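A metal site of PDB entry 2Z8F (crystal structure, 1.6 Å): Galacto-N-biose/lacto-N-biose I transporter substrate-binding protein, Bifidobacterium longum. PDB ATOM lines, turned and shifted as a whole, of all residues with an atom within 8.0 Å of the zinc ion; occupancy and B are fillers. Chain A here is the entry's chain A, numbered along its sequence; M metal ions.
The zinc ion is bound by the side-chain carboxylate (OE1) of Glu 303 (1.9 Å).
The zinc ion is bound by a ring nitrogen (ND1) of His 300, 2.0 Å away.
The zinc ion is bound by OD2 of Asp 12 (2.1 Å).
The zinc ion has three donor atoms within binding distance.
The backbone NH (N) of His 300 lies within hydrogen-bond range of the side-chain hydroxyl (OG) of Ser 298.
Of the 16 residues printed, 3 come within 4 Å of the zinc ion.
Along chain A the residues within 4 Å of the zinc ion span positions 12 to 303.
The nearest printed residue that does not touch the zinc ion is Val 16 (4.2 Å).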
ATOM      1  N   ASP A  11      17.087  27.075  23.899  1.00  0.00           N
ATOM      2  CA  ASP A  11      18.184  26.548  23.043  1.00  0.00           C
ATOM      3  C   ASP A  11      18.157  25.027  22.984  1.00  0.00           C
ATOM      4  O   ASP A  11      17.586  24.373  23.857  1.00  0.00           O
ATOM      5  CB  ASP A  11      19.554  26.988  23.594  1.00  0.00           C
ATOM      6  CG  ASP A  11      20.084  28.274  22.960  1.00  0.00           C
ATOM      7  OD1 ASP A  11      19.479  28.839  22.002  1.00  0.00           O
ATOM      8  OD2 ASP A  11      21.143  28.735  23.434  1.00  0.00           O
ATOM      9  N   ASP A  12      18.812  24.483  21.970  1.00  0.00           N
ATOM     10  CA  ASP A  12      19.049  23.048  21.839  1.00  0.00           C
ATOM     11  C   ASP A  12      19.855  22.540  23.013  1.00  0.00           C
ATOM     12  O   ASP A  12      20.493  23.312  23.736  1.00  0.00           O
ATOM     13  CB  ASP A  12      19.886  22.775  20.587  1.00  0.00           C
ATOM     14  CG  ASP A  12      19.125  22.967  19.310  1.00  0.00           C
ATOM     15  OD1 ASP A  12      17.859  22.955  19.338  1.00  0.00           O
ATOM     16  OD2 ASP A  12      19.810  23.137  18.280  1.00  0.00           O
ATOM     17  N   GLY A  13      19.844  21.222  23.191  1.00  0.00           N
ATOM     18  CA  GLY A  13      20.691  20.556  24.163  1.00  0.00           C
ATOM     19  C   GLY A  13      22.162  20.656  23.775  1.00  0.00           C
ATOM     20  O   GLY A  13      22.492  21.109  22.680  1.00  0.00           O
ATOM     21  N   VAL A  16      23.826  18.251  19.466  1.00  0.00           N
ATOM     22  CA  VAL A  16      22.871  18.054  18.392  1.00  0.00           C
ATOM     23  C   VAL A  16      23.504  17.039  17.461  1.00  0.00           C
ATOM     24  O   VAL A  16      24.699  17.113  17.180  1.00  0.00           O
ATOM     25  CB  VAL A  16      22.563  19.419  17.699  1.00  0.00           C
ATOM     26  CG1 VAL A  16      22.039  19.222  16.289  1.00  0.00           C
ATOM     27  CG2 VAL A  16      21.567  20.211  18.559  1.00  0.00           C
ATOM     28  N   ASN A  17      22.700  16.076  16.989  1.00  0.00           N
ATOM     29  CA  ASN A  17      23.201  15.055  16.092  1.00  0.00           C
ATOM     30  C   ASN A  17      22.534  15.187  14.742  1.00  0.00           C
ATOM     31  O   ASN A  17      21.316  15.143  14.669  1.00  0.00           O
ATOM     32  CB  ASN A  17      22.904  13.677  16.654  1.00  0.00           C
ATOM     33  CG  ASN A  17      23.763  13.342  17.866  1.00  0.00           C
ATOM     34  OD1 ASN A  17      24.934  12.995  17.719  1.00  0.00           O
ATOM     35  ND2 ASN A  17      23.164  13.389  19.050  1.00  0.00           N
ATOM     36  N   ILE A  18      23.376  15.305  13.711  1.00  0.00           N
ATOM     37  CA  ILE A  18      22.975  15.533  12.319  1.00  0.00           C
ATOM     38  C   ILE A  18      23.407  14.331  11.486  1.00  0.00           C
ATOM     39  O   ILE A  18      24.478  13.779  11.702  1.00  0.00           O
ATOM     40  CB  ILE A  18      23.726  16.805  11.759  1.00  0.00           C
ATOM     41  CG1 ILE A  18      23.332  18.052  12.567  1.00  0.00           C
ATOM     42  CG2 ILE A  18      23.532  17.012  10.227  1.00  0.00           C
ATOM     43  CD1 ILE A  18      21.844  18.295  12.624  1.00  0.00           C
ATOM     44  N   ASP A  46      29.411  19.969  19.976  1.00  0.00           N
ATOM     45  CA  ASP A  46      28.048  20.487  20.057  1.00  0.00           C
ATOM     46  C   ASP A  46      27.156  20.145  18.842  1.00  0.00           C
ATOM     47  O   ASP A  46      25.918  20.175  18.952  1.00  0.00           O
ATOM     48  CB  ASP A  46      28.080  22.012  20.279  1.00  0.00           C
ATOM     49  CG  ASP A  46      28.810  22.766  19.171  1.00  0.00           C
ATOM     50  OD1 ASP A  46      30.040  22.530  18.905  1.00  0.00           O
ATOM     51  OD2 ASP A  46      28.178  23.669  18.571  1.00  0.00           O
ATOM     52  N   ILE A  47      27.781  19.853  17.696  1.00  0.00           N
ATOM     53  CA  ILE A  47      27.061  19.433  16.490  1.00  0.00           C
ATOM     54  C   ILE A  47      27.819  18.246  15.865  1.00  0.00           C
ATOM     55  O   ILE A  47      28.811  18.439  15.151  1.00  0.00           O
ATOM     56  CB  ILE A  47      26.955  20.564  15.435  1.00  0.00           C
ATOM     57  CG1 ILE A  47      26.293  21.812  16.013  1.00  0.00           C
ATOM     58  CG2 ILE A  47      26.201  20.046  14.179  1.00  0.00           C
ATOM     59  CD1 ILE A  47      26.630  23.106  15.248  1.00  0.00           C
ATOM     60  N   TYR A 100      18.339  30.533   6.945  1.00  0.00           N
ATOM     61  CA  TYR A 100      19.700  30.052   7.180  1.00  0.00           C
ATOM     62  C   TYR A 100      20.582  30.191   5.948  1.00  0.00           C
ATOM     63  O   TYR A 100      21.687  30.708   6.037  1.00  0.00           O
ATOM     64  CB  TYR A 100      19.709  28.607   7.704  1.00  0.00           C
ATOM     65  CG  TYR A 100      18.758  28.417   8.862  1.00  0.00           C
ATOM     66  CD1 TYR A 100      18.972  29.073  10.076  1.00  0.00           C
ATOM     67  CD2 TYR A 100      17.639  27.581   8.744  1.00  0.00           C
ATOM     68  CE1 TYR A 100      18.102  28.936  11.131  1.00  0.00           C
ATOM     69  CE2 TYR A 100      16.767  27.424   9.805  1.00  0.00           C
ATOM     70  CZ  TYR A 100      17.022  28.087  11.012  1.00  0.00           C
ATOM     71  OH  TYR A 100      16.163  27.924  12.060  1.00  0.00           O
ATOM     72  N   SER A 298      13.705  17.309   9.379  1.00  0.00           N
ATOM     73  CA  SER A 298      14.890  17.615  10.182  1.00  0.00           C
ATOM     74  C   SER A 298      14.518  18.570  11.317  1.00  0.00           C
ATOM     75  O   SER A 298      13.903  19.604  11.085  1.00  0.00           O
ATOM     76  CB  SER A 298      16.019  18.240   9.367  1.00  0.00           C
ATOM     77  OG  SER A 298      17.078  18.624  10.248  1.00  0.00           O
ATOM     78  N   LYS A 299      14.899  18.205  12.529  1.00  0.00           N
ATOM     79  CA  LYS A 299      14.636  19.002  13.733  1.00  0.00           C
ATOM     80  C   LYS A 299      15.670  20.104  13.921  1.00  0.00           C
ATOM     81  O   LYS A 299      15.470  21.011  14.736  1.00  0.00           O
ATOM     82  CB  LYS A 299      14.673  18.082  14.968  1.00  0.00           C
ATOM     83  CG  LYS A 299      13.749  16.848  14.882  1.00  0.00           C
ATOM     84  CD  LYS A 299      12.283  17.262  14.760  1.00  0.00           C
ATOM     85  CE  LYS A 299      11.556  17.187  16.117  1.00  0.00           C
ATOM     86  NZ  LYS A 299      10.386  18.109  16.175  1.00  0.00           N
ATOM     87  N   HIS A 300      16.776  20.025  13.168  1.00  0.00           N
ATOM     88  CA  HIS A 300      17.888  20.938  13.378  1.00  0.00           C
ATOM     89  C   HIS A 300      18.383  21.583  12.102  1.00  0.00           C
ATOM     90  O   HIS A 300      19.552  21.443  11.767  1.00  0.00           O
ATOM     91  CB  HIS A 300      19.019  20.243  14.145  1.00  0.00           C
ATOM     92  CG  HIS A 300      18.614  19.841  15.539  1.00  0.00           C
ATOM     93  ND1 HIS A 300      18.495  20.746  16.562  1.00  0.00           N
ATOM     94  CD2 HIS A 300      18.257  18.635  16.047  1.00  0.00           C
ATOM     95  CE1 HIS A 300      18.083  20.111  17.654  1.00  0.00           C
ATOM     96  NE2 HIS A 300      17.947  18.823  17.365  1.00  0.00           N
ATOM     97  N   PRO A 301      17.483  22.312  11.400  1.00  0.00           N
ATOM     98  CA  PRO A 301      17.910  22.959  10.159  1.00  0.00           C
ATOM     99  C   PRO A 301      19.041  23.968  10.334  1.00  0.00           C
ATOM    100  O   PRO A 301      19.884  24.069   9.456  1.00  0.00           O
ATOM    101  CB  PRO A 301      16.647  23.694   9.683  1.00  0.00           C
ATOM    102  CG  PRO A 301      15.793  23.836  10.902  1.00  0.00           C
ATOM    103  CD  PRO A 301      16.083  22.617  11.734  1.00  0.00           C
ATOM    104  N   LYS A 302      19.071  24.712  11.437  1.00  0.00           N
ATOM    105  CA  LYS A 302      20.147  25.702  11.610  1.00  0.00           C
ATOM    106  C   LYS A 302      21.519  25.052  11.679  1.00  0.00           C
ATOM    107  O   LYS A 302      22.465  25.490  11.024  1.00  0.00           O
ATOM    108  CB  LYS A 302      19.940  26.552  12.861  1.00  0.00           C
ATOM    109  CG  LYS A 302      20.970  27.653  12.945  1.00  0.00           C
ATOM    110  CD  LYS A 302      20.707  28.692  14.006  1.00  0.00           C
ATOM    111  CE  LYS A 302      21.755  29.786  13.894  1.00  0.00           C
ATOM    112  NZ  LYS A 302      21.547  30.965  14.806  1.00  0.00           N
ATOM    113  N   GLU A 303      21.643  24.030  12.504  1.00  0.00           N
ATOM    114  CA  GLU A 303      22.929  23.371  12.651  1.00  0.00           C
ATOM    115  C   GLU A 303      23.289  22.489  11.446  1.00  0.00           C
ATOM    116  O   GLU A 303      24.451  22.374  11.094  1.00  0.00           O
ATOM    117  CB  GLU A 303      22.976  22.581  13.974  1.00  0.00           C
ATOM    118  CG  GLU A 303      22.824  23.442  15.216  1.00  0.00           C
ATOM    119  CD  GLU A 303      21.368  23.749  15.524  1.00  0.00           C
ATOM    120  OE1 GLU A 303      20.501  22.834  15.377  1.00  0.00           O
ATOM    121  OE2 GLU A 303      21.056  24.918  15.921  1.00  0.00           O
ATOM    122  N   ALA A 304      22.295  21.867  10.826  1.00  0.00           N
ATOM    123  CA  ALA A 304      22.538  21.220   9.556  1.00  0.00           C
ATOM    124  C   ALA A 304      23.187  22.174   8.550  1.00  0.00           C
ATOM    125  O   ALA A 304      24.158  21.817   7.880  1.00  0.00           O
ATOM    126  CB  ALA A 304      21.234  20.631   8.999  1.00  0.00           C
HETATM  127 ZN    ZN M   1      18.933  22.721  16.444  1.00  0.00          ZN
